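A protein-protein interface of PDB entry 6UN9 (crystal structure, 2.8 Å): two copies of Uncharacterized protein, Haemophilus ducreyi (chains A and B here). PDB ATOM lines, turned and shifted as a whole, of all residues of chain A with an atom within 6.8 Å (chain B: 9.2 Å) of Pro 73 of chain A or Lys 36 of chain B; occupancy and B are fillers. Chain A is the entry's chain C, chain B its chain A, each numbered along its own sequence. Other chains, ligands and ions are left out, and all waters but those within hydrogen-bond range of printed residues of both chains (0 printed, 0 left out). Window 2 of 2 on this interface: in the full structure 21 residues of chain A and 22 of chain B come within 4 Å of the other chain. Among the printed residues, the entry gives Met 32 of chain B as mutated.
OG of Ser 68 of chain A sits close to OE1 of Glu 69 of chain A, 3.5 Å away.
CB of Ser 68 of chain A touches CD1 of Phe 43 of chain B (3.5 Å). O of Leu 71 of chain A touches CD1 of Leu 39 of chain B, 3.2 Å away. CG of Glu 40 of chain B touches CD1 of Leu 72 of chain A, 3.6 Å away. Pro 73 of chain A touches Lys 36 of chain B (CG to CE, 3.7 Å). OE1 of Glu 40 of chain B touches CG of Pro 73 of chain A, at 3.9 Å. Asn 76 of chain A touches Glu 40 of chain B (CB to CG, 3.5 Å).
Of chain B, only Lys 36 and Glu 40 come within 4 Å of Pro 73 of chain A. Lys 36 of chain B touches one residue of chain A. Leu 72 of chain A touches one residue of chain B. Glu 74 of chain A touches none of the printed residues of chain B. Of the printed residues of chain A, Glu 40 of chain B touches Leu 72, Pro 73 and Asn 76. Of the printed residues of chain B, Asn 76 of chain A touches Glu 40. Of the printed residues of chain A, Phe 43 of chain B touches Ser 68 (3.5 Å). Printed residues of chain B within 4 Å of Leu 71 of chain A: Leu 39. Printed residues of chain A within 4 Å of Leu 39 of chain B: Leu 71 (3.2 Å). Glu 34 of chain B touches none of the printed residues of chain A. Glu 33 of chain B touches none of the printed residues of chain A. The nearest printed residue of chain B that does not touch Asn 76 of chain A is Phe 43 of chain B (4.4 Å).
Of the 9 printed residues of chain A, 5 touch a printed residue of chain B. Along chain A the printed residues that touch a printed residue of chain B span positions 68 to 76. Printed residues of chain B that touch a printed residue of chain A: Lys 36, Leu 39, Glu 40 and Phe 43. Hydrophobic or aromatic side chains of chain B within 4 Å of the printed part of chain A: Leu 39 and Phe 43. Among the printed residues, 6 pairs touch across the chains.
No position is printed for both chains.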
ATOM      1  N   SER A  68     -25.256   8.468   9.146  1.00  0.00           N
ATOM      2  CA  SER A  68     -25.976   8.639   7.888  1.00  0.00           C
ATOM      3  C   SER A  68     -27.253   9.453   8.039  1.00  0.00           C
ATOM      4  O   SER A  68     -27.793   9.907   7.028  1.00  0.00           O
ATOM      5  CB  SER A  68     -26.328   7.297   7.239  1.00  0.00           C
ATOM      6  OG  SER A  68     -26.895   7.488   5.943  1.00  0.00           O
ATOM      7  N   GLU A  69     -27.760   9.654   9.249  1.00  0.00           N
ATOM      8  CA  GLU A  69     -28.907  10.539   9.422  1.00  0.00           C
ATOM      9  C   GLU A  69     -28.680  11.676  10.411  1.00  0.00           C
ATOM     10  O   GLU A  69     -29.507  12.591  10.454  1.00  0.00           O
ATOM     11  CB  GLU A  69     -30.154   9.742   9.835  1.00  0.00           C
ATOM     12  CG  GLU A  69     -31.060   9.368   8.653  1.00  0.00           C
ATOM     13  CD  GLU A  69     -30.374   8.487   7.600  1.00  0.00           C
ATOM     14  OE1 GLU A  69     -29.742   7.461   7.960  1.00  0.00           O
ATOM     15  OE2 GLU A  69     -30.474   8.830   6.399  1.00  0.00           O
ATOM     16  N   LEU A  71     -25.952  13.428   9.938  1.00  0.00           N
ATOM     17  CA  LEU A  71     -25.129  14.285   9.092  1.00  0.00           C
ATOM     18  C   LEU A  71     -25.783  14.565   7.750  1.00  0.00           C
ATOM     19  O   LEU A  71     -25.129  15.081   6.839  1.00  0.00           O
ATOM     20  CB  LEU A  71     -23.752  13.666   8.866  1.00  0.00           C
ATOM     21  CG  LEU A  71     -22.732  13.836   9.991  1.00  0.00           C
ATOM     22  CD1 LEU A  71     -22.954  12.840  11.143  1.00  0.00           C
ATOM     23  CD2 LEU A  71     -21.317  13.729   9.441  1.00  0.00           C
ATOM     24  N   LEU A  72     -27.071  14.270   7.612  1.00  0.00           N
ATOM     25  CA  LEU A  72     -27.591  14.221   6.260  1.00  0.00           C
ATOM     26  C   LEU A  72     -29.084  14.497   6.253  1.00  0.00           C
ATOM     27  O   LEU A  72     -29.796  13.967   7.116  1.00  0.00           O
ATOM     28  CB  LEU A  72     -27.293  12.843   5.661  1.00  0.00           C
ATOM     29  CG  LEU A  72     -27.722  12.573   4.228  1.00  0.00           C
ATOM     30  CD1 LEU A  72     -26.498  12.513   3.313  1.00  0.00           C
ATOM     31  CD2 LEU A  72     -28.488  11.269   4.233  1.00  0.00           C
ATOM     32  N   PRO A  73     -29.589  15.300   5.315  1.00  0.00           N
ATOM     33  CA  PRO A  73     -31.034  15.557   5.247  1.00  0.00           C
ATOM     34  C   PRO A  73     -31.845  14.275   5.149  1.00  0.00           C
ATOM     35  O   PRO A  73     -31.332  13.163   4.979  1.00  0.00           O
ATOM     36  CB  PRO A  73     -31.195  16.393   3.974  1.00  0.00           C
ATOM     37  CG  PRO A  73     -29.921  16.188   3.199  1.00  0.00           C
ATOM     38  CD  PRO A  73     -28.867  16.006   4.241  1.00  0.00           C
ATOM     39  N   GLU A  74     -33.161  14.466   5.241  1.00  0.00           N
ATOM     40  CA  GLU A  74     -34.132  13.379   5.241  1.00  0.00           C
ATOM     41  C   GLU A  74     -34.356  12.787   3.854  1.00  0.00           C
ATOM     42  O   GLU A  74     -35.036  11.759   3.738  1.00  0.00           O
ATOM     43  CB  GLU A  74     -35.470  13.875   5.815  1.00  0.00           C
ATOM     44  CG  GLU A  74     -35.419  14.419   7.257  1.00  0.00           C
ATOM     45  CD  GLU A  74     -34.661  15.741   7.398  1.00  0.00           C
ATOM     46  OE1 GLU A  74     -33.674  15.782   8.167  1.00  0.00           O
ATOM     47  OE2 GLU A  74     -35.043  16.732   6.735  1.00  0.00           O
ATOM     48  N   SER A  75     -33.798  13.404   2.810  1.00  0.00           N
ATOM     49  CA  SER A  75     -34.110  13.054   1.431  1.00  0.00           C
ATOM     50  C   SER A  75     -33.236  11.933   0.878  1.00  0.00           C
ATOM     51  O   SER A  75     -33.543  11.399  -0.192  1.00  0.00           O
ATOM     52  CB  SER A  75     -33.989  14.299   0.541  1.00  0.00           C
ATOM     53  OG  SER A  75     -34.853  14.221  -0.579  1.00  0.00           O
ATOM     54  N   ASN A  76     -32.163  11.569   1.570  1.00  0.00           N
ATOM     55  CA  ASN A  76     -31.383  10.384   1.237  1.00  0.00           C
ATOM     56  C   ASN A  76     -31.698   9.284   2.250  1.00  0.00           C
ATOM     57  O   ASN A  76     -30.870   8.893   3.083  1.00  0.00           O
ATOM     58  CB  ASN A  76     -29.881  10.724   1.189  1.00  0.00           C
ATOM     59  CG  ASN A  76     -29.021   9.563   0.658  1.00  0.00           C
ATOM     60  OD1 ASN A  76     -29.348   8.940  -0.355  1.00  0.00           O
ATOM     61  ND2 ASN A  76     -27.907   9.288   1.333  1.00  0.00           N
ATOM     62  N   GLN A  77     -32.943   8.800   2.197  1.00  0.00           N
ATOM     63  CA  GLN A  77     -33.338   7.588   2.913  1.00  0.00           C
ATOM     64  C   GLN A  77     -32.778   6.408   2.130  1.00  0.00           C
ATOM     65  O   GLN A  77     -33.479   5.721   1.381  1.00  0.00           O
ATOM     66  CB  GLN A  77     -34.854   7.498   3.060  1.00  0.00           C
ATOM     67  CG  GLN A  77     -35.460   8.582   3.928  1.00  0.00           C
ATOM     68  CD  GLN A  77     -36.762   9.113   3.367  1.00  0.00           C
ATOM     69  OE1 GLN A  77     -37.457   8.421   2.621  1.00  0.00           O
ATOM     70  NE2 GLN A  77     -37.093  10.354   3.711  1.00  0.00           N
ATOM     71  N   ALA B  28     -19.480  30.085  -0.696  1.00  0.00           N
ATOM     72  CA  ALA B  28     -19.802  29.241   0.446  1.00  0.00           C
ATOM     73  C   ALA B  28     -21.078  28.443   0.205  1.00  0.00           C
ATOM     74  O   ALA B  28     -21.197  27.318   0.674  1.00  0.00           O
ATOM     75  CB  ALA B  28     -19.931  30.088   1.716  1.00  0.00           C
ATOM     76  N   GLU B  29     -22.063  29.001  -0.489  1.00  0.00           N
ATOM     77  CA  GLU B  29     -23.269  28.217  -0.720  1.00  0.00           C
ATOM     78  C   GLU B  29     -23.019  27.112  -1.746  1.00  0.00           C
ATOM     79  O   GLU B  29     -23.555  26.008  -1.604  1.00  0.00           O
ATOM     80  CB  GLU B  29     -24.424  29.137  -1.135  1.00  0.00           C
ATOM     81  CG  GLU B  29     -25.014  29.914   0.055  1.00  0.00           C
ATOM     82  CD  GLU B  29     -26.133  30.898  -0.316  1.00  0.00           C
ATOM     83  OE1 GLU B  29     -26.448  31.044  -1.525  1.00  0.00           O
ATOM     84  OE2 GLU B  29     -26.697  31.524   0.621  1.00  0.00           O
ATOM     85  N   ALA B  30     -22.200  27.378  -2.768  1.00  0.00           N
ATOM     86  CA  ALA B  30     -21.833  26.331  -3.714  1.00  0.00           C
ATOM     87  C   ALA B  30     -20.985  25.261  -3.042  1.00  0.00           C
ATOM     88  O   ALA B  30     -21.108  24.071  -3.347  1.00  0.00           O
ATOM     89  CB  ALA B  30     -21.078  26.926  -4.901  1.00  0.00           C
ATOM     90  N   LYS B  31     -20.104  25.670  -2.138  1.00  0.00           N
ATOM     91  CA  LYS B  31     -19.247  24.706  -1.471  1.00  0.00           C
ATOM     92  C   LYS B  31     -20.083  23.753  -0.617  1.00  0.00           C
ATOM     93  O   LYS B  31     -19.868  22.531  -0.636  1.00  0.00           O
ATOM     94  CB  LYS B  31     -18.196  25.464  -0.651  1.00  0.00           C
ATOM     95  CG  LYS B  31     -16.940  24.717  -0.294  1.00  0.00           C
ATOM     96  CD  LYS B  31     -17.070  24.168   1.121  1.00  0.00           C
ATOM     97  CE  LYS B  31     -16.059  23.063   1.460  1.00  0.00           C
ATOM     98  NZ  LYS B  31     -16.358  22.479   2.832  1.00  0.00           N
ATOM     99  N   MET B  32     -21.091  24.291   0.072  1.00  0.00           N
ATOM    100  CA  MET B  32     -21.931  23.546   1.006  1.00  0.00           C
ATOM    101  C   MET B  32     -22.834  22.511   0.386  1.00  0.00           C
ATOM    102  O   MET B  32     -23.229  21.559   1.062  1.00  0.00           O
ATOM    103  CB  MET B  32     -22.827  24.479   1.795  1.00  0.00           C
ATOM    104  CG  MET B  32     -22.142  25.191   2.927  1.00  0.00           C
ATOM    105  SD  MET B  32     -23.452  25.984   4.124  1.00  0.00           S
ATOM    106  CE  MET B  32     -24.645  26.865   2.846  1.00  0.00           C
ATOM    107  N   GLU B  33     -23.209  22.776  -0.871  1.00  0.00           N
ATOM    108  CA  GLU B  33     -24.096  21.908  -1.689  1.00  0.00           C
ATOM    109  C   GLU B  33     -23.222  20.848  -2.350  1.00  0.00           C
ATOM    110  O   GLU B  33     -23.714  19.740  -2.582  1.00  0.00           O
ATOM    111  CB  GLU B  33     -24.859  22.715  -2.732  1.00  0.00           C
ATOM    112  CG  GLU B  33     -26.003  21.935  -3.339  1.00  0.00           C
ATOM    113  CD  GLU B  33     -27.078  22.789  -3.981  1.00  0.00           C
ATOM    114  OE1 GLU B  33     -27.897  22.230  -4.736  1.00  0.00           O
ATOM    115  OE2 GLU B  33     -27.091  24.008  -3.724  1.00  0.00           O
ATOM    116  N   GLU B  34     -22.010  21.228  -2.747  1.00  0.00           N
ATOM    117  CA  GLU B  34     -21.056  20.214  -3.170  1.00  0.00           C
ATOM    118  C   GLU B  34     -20.847  19.201  -2.050  1.00  0.00           C
ATOM    119  O   GLU B  34     -21.078  18.001  -2.223  1.00  0.00           O
ATOM    120  CB  GLU B  34     -19.725  20.853  -3.543  1.00  0.00           C
ATOM    121  CG  GLU B  34     -18.958  20.138  -4.667  1.00  0.00           C
ATOM    122  CD  GLU B  34     -17.484  20.568  -4.751  1.00  0.00           C
ATOM    123  OE1 GLU B  34     -16.698  20.235  -3.820  1.00  0.00           O
ATOM    124  OE2 GLU B  34     -17.120  21.256  -5.741  1.00  0.00           O
ATOM    125  N   GLN B  35     -20.421  19.689  -0.887  1.00  0.00           N
ATOM    126  CA  GLN B  35     -20.259  18.881   0.315  1.00  0.00           C
ATOM    127  C   GLN B  35     -21.501  18.052   0.649  1.00  0.00           C
ATOM    128  O   GLN B  35     -21.379  17.031   1.336  1.00  0.00           O
ATOM    129  CB  GLN B  35     -19.901  19.816   1.488  1.00  0.00           C
ATOM    130  CG  GLN B  35     -19.342  19.135   2.724  1.00  0.00           C
ATOM    131  CD  GLN B  35     -17.847  18.878   2.635  1.00  0.00           C
ATOM    132  OE1 GLN B  35     -17.342  17.873   3.141  1.00  0.00           O
ATOM    133  NE2 GLN B  35     -17.132  19.791   1.997  1.00  0.00           N
ATOM    134  N   LYS B  36     -22.687  18.467   0.193  1.00  0.00           N
ATOM    135  CA  LYS B  36     -23.909  17.750   0.541  1.00  0.00           C
ATOM    136  C   LYS B  36     -24.147  16.576  -0.393  1.00  0.00           C
ATOM    137  O   LYS B  36     -24.545  15.498   0.055  1.00  0.00           O
ATOM    138  CB  LYS B  36     -25.099  18.700   0.515  1.00  0.00           C
ATOM    139  CG  LYS B  36     -26.471  18.065   0.644  1.00  0.00           C
ATOM    140  CD  LYS B  36     -27.470  19.107   1.187  1.00  0.00           C
ATOM    141  CE  LYS B  36     -28.921  18.788   0.827  1.00  0.00           C
ATOM    142  NZ  LYS B  36     -29.099  18.638  -0.654  1.00  0.00           N
ATOM    143  N   GLN B  37     -23.910  16.752  -1.686  1.00  0.00           N
ATOM    144  CA  GLN B  37     -24.094  15.659  -2.622  1.00  0.00           C
ATOM    145  C   GLN B  37     -22.830  14.812  -2.791  1.00  0.00           C
ATOM    146  O   GLN B  37     -22.784  13.964  -3.691  1.00  0.00           O
ATOM    147  CB  GLN B  37     -24.595  16.185  -3.973  1.00  0.00           C
ATOM    148  CG  GLN B  37     -23.542  16.768  -4.896  1.00  0.00           C
ATOM    149  CD  GLN B  37     -24.124  17.133  -6.254  1.00  0.00           C
ATOM    150  OE1 GLN B  37     -25.240  17.656  -6.344  1.00  0.00           O
ATOM    151  NE2 GLN B  37     -23.377  16.854  -7.316  1.00  0.00           N
ATOM    152  N   GLN B  38     -21.807  15.014  -1.953  1.00  0.00           N
ATOM    153  CA  GLN B  38     -20.752  14.024  -1.834  1.00  0.00           C
ATOM    154  C   GLN B  38     -20.730  13.388  -0.457  1.00  0.00           C
ATOM    155  O   GLN B  38     -19.875  12.533  -0.197  1.00  0.00           O
ATOM    156  CB  GLN B  38     -19.378  14.607  -2.199  1.00  0.00           C
ATOM    157  CG  GLN B  38     -18.854  15.744  -1.355  1.00  0.00           C
ATOM    158  CD  GLN B  38     -17.694  16.511  -2.042  1.00  0.00           C
ATOM    159  OE1 GLN B  38     -17.291  16.198  -3.182  1.00  0.00           O
ATOM    160  NE2 GLN B  38     -17.170  17.533  -1.349  1.00  0.00           N
ATOM    161  N   LEU B  39     -21.652  13.782   0.424  1.00  0.00           N
ATOM    162  CA  LEU B  39     -22.042  12.928   1.540  1.00  0.00           C
ATOM    163  C   LEU B  39     -23.076  11.907   1.081  1.00  0.00           C
ATOM    164  O   LEU B  39     -22.949  10.710   1.356  1.00  0.00           O
ATOM    165  CB  LEU B  39     -22.599  13.770   2.691  1.00  0.00           C
ATOM    166  CG  LEU B  39     -21.715  14.018   3.905  1.00  0.00           C
ATOM    167  CD1 LEU B  39     -22.601  14.469   5.032  1.00  0.00           C
ATOM    168  CD2 LEU B  39     -20.899  12.779   4.336  1.00  0.00           C
ATOM    169  N   GLU B  40     -24.102  12.373   0.360  1.00  0.00           N
ATOM    170  CA  GLU B  40     -25.081  11.467  -0.224  1.00  0.00           C
ATOM    171  C   GLU B  40     -24.413  10.408  -1.086  1.00  0.00           C
ATOM    172  O   GLU B  40     -24.926   9.294  -1.191  1.00  0.00           O
ATOM    173  CB  GLU B  40     -26.120  12.255  -1.036  1.00  0.00           C
ATOM    174  CG  GLU B  40     -27.332  12.703  -0.195  1.00  0.00           C
ATOM    175  CD  GLU B  40     -28.227  13.749  -0.867  1.00  0.00           C
ATOM    176  OE1 GLU B  40     -29.122  14.290  -0.168  1.00  0.00           O
ATOM    177  OE2 GLU B  40     -28.039  14.030  -2.074  1.00  0.00           O
ATOM    178  N   ARG B  41     -23.272  10.735  -1.702  1.00  0.00           N
ATOM    179  CA  ARG B  41     -22.529   9.743  -2.474  1.00  0.00           C
ATOM    180  C   ARG B  41     -21.810   8.765  -1.554  1.00  0.00           C
ATOM    181  O   ARG B  41     -21.699   7.575  -1.866  1.00  0.00           O
ATOM    182  CB  ARG B  41     -21.540  10.444  -3.416  1.00  0.00           C
ATOM    183  CG  ARG B  41     -20.292   9.651  -3.826  1.00  0.00           C
ATOM    184  CD  ARG B  41     -20.598   8.507  -4.813  1.00  0.00           C
ATOM    185  NE  ARG B  41     -19.443   8.184  -5.656  1.00  0.00           N
ATOM    186  CZ  ARG B  41     -19.248   8.681  -6.878  1.00  0.00           C
ATOM    187  NH1 ARG B  41     -20.136   9.516  -7.409  1.00  0.00           N
ATOM    188  NH2 ARG B  41     -18.170   8.344  -7.577  1.00  0.00           N
ATOM    189  N   HIS B  42     -21.345   9.243  -0.403  1.00  0.00           N
ATOM    190  CA  HIS B  42     -20.515   8.419   0.455  1.00  0.00           C
ATOM    191  C   HIS B  42     -21.334   7.390   1.217  1.00  0.00           C
ATOM    192  O   HIS B  42     -20.950   6.223   1.274  1.00  0.00           O
ATOM    193  CB  HIS B  42     -19.742   9.320   1.395  1.00  0.00           C
ATOM    194  CG  HIS B  42     -19.276   8.652   2.646  1.00  0.00           C
ATOM    195  ND1 HIS B  42     -17.994   8.174   2.798  1.00  0.00           N
ATOM    196  CD2 HIS B  42     -19.910   8.427   3.824  1.00  0.00           C
ATOM    197  CE1 HIS B  42     -17.859   7.678   4.017  1.00  0.00           C
ATOM    198  NE2 HIS B  42     -19.007   7.819   4.659  1.00  0.00           N
ATOM    199  N   PHE B  43     -22.463   7.791   1.791  1.00  0.00           N
ATOM    200  CA  PHE B  43     -23.348   6.849   2.451  1.00  0.00           C
ATOM    201  C   PHE B  43     -24.118   5.970   1.482  1.00  0.00           C
ATOM    202  O   PHE B  43     -24.748   5.005   1.918  1.00  0.00           O
ATOM    203  CB  PHE B  43     -24.336   7.585   3.359  1.00  0.00           C
ATOM    204  CG  PHE B  43     -23.698   8.173   4.562  1.00  0.00           C
ATOM    205  CD1 PHE B  43     -23.211   7.362   5.559  1.00  0.00           C
ATOM    206  CD2 PHE B  43     -23.549   9.545   4.686  1.00  0.00           C
ATOM    207  CE1 PHE B  43     -22.599   7.885   6.661  1.00  0.00           C
ATOM    208  CE2 PHE B  43     -22.937  10.090   5.797  1.00  0.00           C
ATOM    209  CZ  PHE B  43     -22.457   9.253   6.786  1.00  0.00           C
